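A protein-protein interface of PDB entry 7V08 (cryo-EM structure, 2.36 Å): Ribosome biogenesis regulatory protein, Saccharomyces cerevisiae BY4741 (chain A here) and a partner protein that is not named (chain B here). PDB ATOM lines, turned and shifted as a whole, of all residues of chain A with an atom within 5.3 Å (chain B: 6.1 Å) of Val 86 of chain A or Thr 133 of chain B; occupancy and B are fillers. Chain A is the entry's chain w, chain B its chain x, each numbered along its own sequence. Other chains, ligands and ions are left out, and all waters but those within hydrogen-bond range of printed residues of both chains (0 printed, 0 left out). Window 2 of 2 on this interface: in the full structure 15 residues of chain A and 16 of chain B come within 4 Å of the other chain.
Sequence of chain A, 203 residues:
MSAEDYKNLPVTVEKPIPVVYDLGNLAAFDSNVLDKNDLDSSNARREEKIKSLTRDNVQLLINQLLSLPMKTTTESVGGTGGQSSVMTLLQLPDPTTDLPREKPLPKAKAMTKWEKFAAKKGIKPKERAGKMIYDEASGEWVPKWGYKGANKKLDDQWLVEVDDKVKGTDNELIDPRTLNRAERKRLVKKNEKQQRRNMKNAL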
ATOM      1  N   SER A  76     -12.307  -9.209 -30.776  1.00  0.00           N
ATOM      2  CA  SER A  76     -12.067 -10.191 -29.734  1.00  0.00           C
ATOM      3  C   SER A  76     -11.007  -9.681 -28.763  1.00  0.00           C
ATOM      4  O   SER A  76     -10.426  -8.608 -28.934  1.00  0.00           O
ATOM      5  CB  SER A  76     -11.639 -11.522 -30.348  1.00  0.00           C
ATOM      6  OG  SER A  76     -12.533 -11.925 -31.361  1.00  0.00           O
ATOM      7  N   VAL A  77     -10.740 -10.478 -27.733  1.00  0.00           N
ATOM      8  CA  VAL A  77      -9.715 -10.161 -26.748  1.00  0.00           C
ATOM      9  C   VAL A  77      -8.344 -10.399 -27.361  1.00  0.00           C
ATOM     10  O   VAL A  77      -8.224 -10.998 -28.434  1.00  0.00           O
ATOM     11  CB  VAL A  77      -9.897 -10.998 -25.473  1.00  0.00           C
ATOM     12  CG1 VAL A  77     -11.266 -10.754 -24.864  1.00  0.00           C
ATOM     13  CG2 VAL A  77      -9.712 -12.459 -25.788  1.00  0.00           C
ATOM     14  N   SER A  84     -13.409  -5.307 -25.467  1.00  0.00           N
ATOM     15  CA  SER A  84     -13.757  -6.570 -26.091  1.00  0.00           C
ATOM     16  C   SER A  84     -15.251  -6.615 -26.402  1.00  0.00           C
ATOM     17  O   SER A  84     -16.034  -5.773 -25.958  1.00  0.00           O
ATOM     18  CB  SER A  84     -13.347  -7.741 -25.196  1.00  0.00           C
ATOM     19  OG  SER A  84     -14.013  -7.698 -23.950  1.00  0.00           O
ATOM     20  N   SER A  85     -15.633  -7.634 -27.175  1.00  0.00           N
ATOM     21  CA  SER A  85     -16.976  -7.709 -27.744  1.00  0.00           C
ATOM     22  C   SER A  85     -18.047  -7.799 -26.667  1.00  0.00           C
ATOM     23  O   SER A  85     -19.134  -7.229 -26.815  1.00  0.00           O
ATOM     24  CB  SER A  85     -17.063  -8.907 -28.685  1.00  0.00           C
ATOM     25  OG  SER A  85     -18.404  -9.256 -28.966  1.00  0.00           O
ATOM     26  N   VAL A  86     -17.760  -8.508 -25.574  1.00  0.00           N
ATOM     27  CA  VAL A  86     -18.741  -8.690 -24.516  1.00  0.00           C
ATOM     28  C   VAL A  86     -18.910  -7.439 -23.663  1.00  0.00           C
ATOM     29  O   VAL A  86     -19.904  -7.317 -22.940  1.00  0.00           O
ATOM     30  CB  VAL A  86     -18.350  -9.907 -23.658  1.00  0.00           C
ATOM     31  CG1 VAL A  86     -18.492 -11.185 -24.471  1.00  0.00           C
ATOM     32  CG2 VAL A  86     -16.926  -9.769 -23.158  1.00  0.00           C
ATOM     33  N   MET A  87     -17.969  -6.499 -23.732  1.00  0.00           N
ATOM     34  CA  MET A  87     -18.019  -5.296 -22.911  1.00  0.00           C
ATOM     35  C   MET A  87     -18.791  -4.183 -23.609  1.00  0.00           C
ATOM     36  O   MET A  87     -18.690  -4.012 -24.825  1.00  0.00           O
ATOM     37  CB  MET A  87     -16.608  -4.814 -22.590  1.00  0.00           C
ATOM     38  CG  MET A  87     -15.799  -5.787 -21.775  1.00  0.00           C
ATOM     39  SD  MET A  87     -14.135  -5.189 -21.453  1.00  0.00           S
ATOM     40  CE  MET A  87     -14.496  -3.615 -20.685  1.00  0.00           C
ATOM     41  N   THR A  88     -19.557  -3.425 -22.833  1.00  0.00           N
ATOM     42  CA  THR A  88     -20.252  -2.238 -23.314  1.00  0.00           C
ATOM     43  C   THR A  88     -19.849  -1.056 -22.446  1.00  0.00           C
ATOM     44  O   THR A  88     -20.041  -1.090 -21.226  1.00  0.00           O
ATOM     45  CB  THR A  88     -21.765  -2.439 -23.281  1.00  0.00           C
ATOM     46  OG1 THR A  88     -22.139  -3.425 -24.253  1.00  0.00           O
ATOM     47  CG2 THR A  88     -22.484  -1.145 -23.574  1.00  0.00           C
ATOM     48  N   PRO B 131     -21.731 -16.758 -26.323  1.00  0.00           N
ATOM     49  CA  PRO B 131     -20.930 -16.592 -27.538  1.00  0.00           C
ATOM     50  C   PRO B 131     -19.471 -16.936 -27.299  1.00  0.00           C
ATOM     51  O   PRO B 131     -18.918 -16.704 -26.223  1.00  0.00           O
ATOM     52  CB  PRO B 131     -21.100 -15.106 -27.875  1.00  0.00           C
ATOM     53  CG  PRO B 131     -22.353 -14.700 -27.192  1.00  0.00           C
ATOM     54  CD  PRO B 131     -22.417 -15.515 -25.938  1.00  0.00           C
ATOM     55  N   VAL B 132     -18.846 -17.504 -28.321  1.00  0.00           N
ATOM     56  CA  VAL B 132     -17.413 -17.760 -28.280  1.00  0.00           C
ATOM     57  C   VAL B 132     -16.681 -16.473 -28.625  1.00  0.00           C
ATOM     58  O   VAL B 132     -17.074 -15.746 -29.543  1.00  0.00           O
ATOM     59  CB  VAL B 132     -17.032 -18.906 -29.228  1.00  0.00           C
ATOM     60  CG1 VAL B 132     -17.412 -20.230 -28.608  1.00  0.00           C
ATOM     61  CG2 VAL B 132     -17.725 -18.739 -30.562  1.00  0.00           C
ATOM     62  N   THR B 133     -15.639 -16.161 -27.862  1.00  0.00           N
ATOM     63  CA  THR B 133     -15.006 -14.854 -27.944  1.00  0.00           C
ATOM     64  C   THR B 133     -13.501 -14.903 -28.134  1.00  0.00           C
ATOM     65  O   THR B 133     -12.902 -13.872 -28.455  1.00  0.00           O
ATOM     66  CB  THR B 133     -15.323 -14.043 -26.685  1.00  0.00           C
ATOM     67  OG1 THR B 133     -14.969 -14.806 -25.526  1.00  0.00           O
ATOM     68  CG2 THR B 133     -16.802 -13.687 -26.630  1.00  0.00           C
ATOM     69  N   ARG B 134     -12.870 -16.056 -27.954  1.00  0.00           N
ATOM     70  CA  ARG B 134     -11.417 -16.109 -27.963  1.00  0.00           C
ATOM     71  C   ARG B 134     -10.982 -17.499 -28.381  1.00  0.00           C
ATOM     72  O   ARG B 134     -11.704 -18.477 -28.189  1.00  0.00           O
ATOM     73  CB  ARG B 134     -10.838 -15.756 -26.589  1.00  0.00           C
ATOM     74  CG  ARG B 134     -11.564 -16.402 -25.420  1.00  0.00           C
ATOM     75  CD  ARG B 134     -11.257 -15.701 -24.105  1.00  0.00           C
ATOM     76  NE  ARG B 134     -11.812 -16.422 -22.968  1.00  0.00           N
ATOM     77  CZ  ARG B 134     -11.223 -17.455 -22.382  1.00  0.00           C
ATOM     78  NH1 ARG B 134     -10.050 -17.904 -22.792  1.00  0.00           N
ATOM     79  NH2 ARG B 134     -11.826 -18.053 -21.361  1.00  0.00           N
ATOM     80  N   SER B 135      -9.781 -17.575 -28.942  1.00  0.00           N
ATOM     81  CA  SER B 135      -9.207 -18.843 -29.357  1.00  0.00           C
ATOM     82  C   SER B 135      -8.640 -19.535 -28.129  1.00  0.00           C
ATOM     83  O   SER B 135      -7.647 -19.072 -27.556  1.00  0.00           O
ATOM     84  CB  SER B 135      -8.120 -18.637 -30.410  1.00  0.00           C
ATOM     85  OG  SER B 135      -7.685 -19.878 -30.947  1.00  0.00           O
ATOM     86  N   VAL B 480     -19.417 -11.078 -32.908  1.00  0.00           N
ATOM     87  CA  VAL B 480     -17.976 -11.001 -32.669  1.00  0.00           C
ATOM     88  C   VAL B 480     -17.225 -11.606 -33.850  1.00  0.00           C
ATOM     89  O   VAL B 480     -17.553 -12.695 -34.326  1.00  0.00           O
ATOM     90  CB  VAL B 480     -17.596 -11.671 -31.326  1.00  0.00           C
ATOM     91  CG1 VAL B 480     -18.339 -12.966 -31.134  1.00  0.00           C
ATOM     92  CG2 VAL B 480     -16.093 -11.888 -31.213  1.00  0.00           C
ATOM     93  N   ASP B 481     -16.212 -10.886 -34.323  1.00  0.00           N
ATOM     94  CA  ASP B 481     -15.336 -11.345 -35.393  1.00  0.00           C
ATOM     95  C   ASP B 481     -14.089 -11.971 -34.783  1.00  0.00           C
ATOM     96  O   ASP B 481     -13.461 -11.375 -33.904  1.00  0.00           O
ATOM     97  CB  ASP B 481     -14.966 -10.185 -36.318  1.00  0.00           C
ATOM     98  CG  ASP B 481     -13.915 -10.557 -37.343  1.00  0.00           C
ATOM     99  OD1 ASP B 481     -14.172 -11.471 -38.155  1.00  0.00           O
ATOM    100  OD2 ASP B 481     -12.838  -9.925 -37.345  1.00  0.00           O
ATOM    101  N   LEU B 482     -13.743 -13.174 -35.235  1.00  0.00           N
ATOM    102  CA  LEU B 482     -12.642 -13.946 -34.664  1.00  0.00           C
ATOM    103  C   LEU B 482     -11.555 -14.163 -35.708  1.00  0.00           C
ATOM    104  O   LEU B 482     -11.705 -15.020 -36.600  1.00  0.00           O
ATOM    105  CB  LEU B 482     -13.150 -15.284 -34.131  1.00  0.00           C
ATOM    106  CG  LEU B 482     -14.336 -15.258 -33.161  1.00  0.00           C
ATOM    107  CD1 LEU B 482     -14.989 -16.629 -33.083  1.00  0.00           C
ATOM    108  CD2 LEU B 482     -13.908 -14.805 -31.779  1.00  0.00           C
ATOM    109  N   TRP B 513     -12.165 -22.613 -29.891  1.00  0.00           N
ATOM    110  CA  TRP B 513     -12.631 -21.298 -29.473  1.00  0.00           C
ATOM    111  C   TRP B 513     -13.681 -21.447 -28.382  1.00  0.00           C
ATOM    112  O   TRP B 513     -14.551 -22.321 -28.464  1.00  0.00           O
ATOM    113  CB  TRP B 513     -13.253 -20.520 -30.643  1.00  0.00           C
ATOM    114  CG  TRP B 513     -12.503 -20.556 -31.937  1.00  0.00           C
ATOM    115  CD1 TRP B 513     -12.487 -21.570 -32.849  1.00  0.00           C
ATOM    116  CD2 TRP B 513     -11.700 -19.509 -32.490  1.00  0.00           C
ATOM    117  NE1 TRP B 513     -11.701 -21.231 -33.918  1.00  0.00           N
ATOM    118  CE2 TRP B 513     -11.206 -19.968 -33.722  1.00  0.00           C
ATOM    119  CE3 TRP B 513     -11.340 -18.232 -32.056  1.00  0.00           C
ATOM    120  CZ2 TRP B 513     -10.374 -19.194 -34.527  1.00  0.00           C
ATOM    121  CZ3 TRP B 513     -10.511 -17.468 -32.852  1.00  0.00           C
ATOM    122  CH2 TRP B 513     -10.042 -17.951 -34.076  1.00  0.00           C
ATOM    123  N   THR B 514     -13.622 -20.564 -27.384  1.00  0.00           N
ATOM    124  CA  THR B 514     -14.514 -20.605 -26.230  1.00  0.00           C
ATOM    125  C   THR B 514     -14.978 -19.201 -25.856  1.00  0.00           C
ATOM    126  O   THR B 514     -14.569 -18.200 -26.451  1.00  0.00           O
ATOM    127  CB  THR B 514     -13.830 -21.259 -25.021  1.00  0.00           C
ATOM    128  OG1 THR B 514     -14.757 -21.341 -23.935  1.00  0.00           O
ATOM    129  CG2 THR B 514     -12.635 -20.443 -24.579  1.00  0.00           C
ATOM    130  N   HIS B 515     -15.843 -19.142 -24.847  1.00  0.00           N
ATOM    131  CA  HIS B 515     -16.298 -17.882 -24.262  1.00  0.00           C
ATOM    132  C   HIS B 515     -15.206 -17.243 -23.406  1.00  0.00           C
ATOM    133  O   HIS B 515     -14.800 -16.103 -23.636  1.00  0.00           O
ATOM    134  CB  HIS B 515     -17.556 -18.116 -23.420  1.00  0.00           C
ATOM    135  CG  HIS B 515     -18.115 -16.875 -22.796  1.00  0.00           C
ATOM    136  ND1 HIS B 515     -19.013 -16.054 -23.445  1.00  0.00           N
ATOM    137  CD2 HIS B 515     -17.911 -16.320 -21.578  1.00  0.00           C
ATOM    138  CE1 HIS B 515     -19.338 -15.049 -22.654  1.00  0.00           C
ATOM    139  NE2 HIS B 515     -18.683 -15.186 -21.515  1.00  0.00           N
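The side-chain hydroxyl (OG) of Ser 76 of chain A lies within hydrogen-bond range of the backbone carbonyl oxygen (O) of Asp 481 of chain B, 2.8 Å away.
The backbone carbonyl oxygen (O) of Thr 514 of chain B lies within hydrogen-bond range of the backbone NH (N) of Thr 133 of chain B (2.7 Å). O of Arg 134 of chain B lies within hydrogen-bond range of N of Thr 514 of chain B, at 2.9 Å. The guanidinium group (NE) of Arg 134 of chain B is in hydrogen-bond range of the backbone carbonyl oxygen (O) of His 515 of chain B, at 3.1 Å.
Among the printed residues, merely in contact across the chains: Ser 76 of chain A with Thr 133 of chain B, Ser 76 of chain A with Val 480 of chain B, Ser 76 of chain A with Leu 482 of chain B, Val 77 of chain A with Arg 134 of chain B, Ser 85 of chain A with Val 480 of chain B and Val 86 of chain A with Thr 133 of chain B.
Of chain B, only Thr 133 comes within 4 Å of Val 86 of chain A. Of chain A, only Ser 76 and Val 86 come within 4 Å of Thr 133 of chain B. Of the printed residues of chain A, Val 480 of chain B touches Ser 76 and Ser 85. Printed residues of chain B within 4 Å of Val 77 of chain A: Arg 134 (3.6 Å). Printed residues of chain B within 4 Å of Ser 76 of chain A: Thr 133 (3.3 Å), Val 480 (3.6 Å), Asp 481 (2.8 Å) and Leu 482 (3.2 Å). Of the printed residues of chain A, Asp 481 of chain B touches Ser 76 (2.8 Å). Printed residues of chain A within 4 Å of Leu 482 of chain B: Ser 76. Trp 513 of chain B touches none of the printed residues of chain A. Pro 131 of chain B touches none of the printed residues of chain A. The nearest residue of chain B that does not touch Val 86 of chain A is His 515 of chain B (4.4 Å). The nearest printed residue of chain B that does not touch Ser 76 of chain A is Arg 134 of chain B (5.2 Å).
Of the 7 printed residues of chain A, 4 touch a printed residue of chain B. Of the 11 printed residues of chain B, 5 touch a printed residue of chain A. Printed residues of chain B that touch a printed residue of chain A: Thr 133, Arg 134, Val 480, Asp 481 and Leu 482. Among the printed residues, no Asp or Glu carboxylate lies within 4 Å of a Lys or Arg side-chain nitrogen of the other chain.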
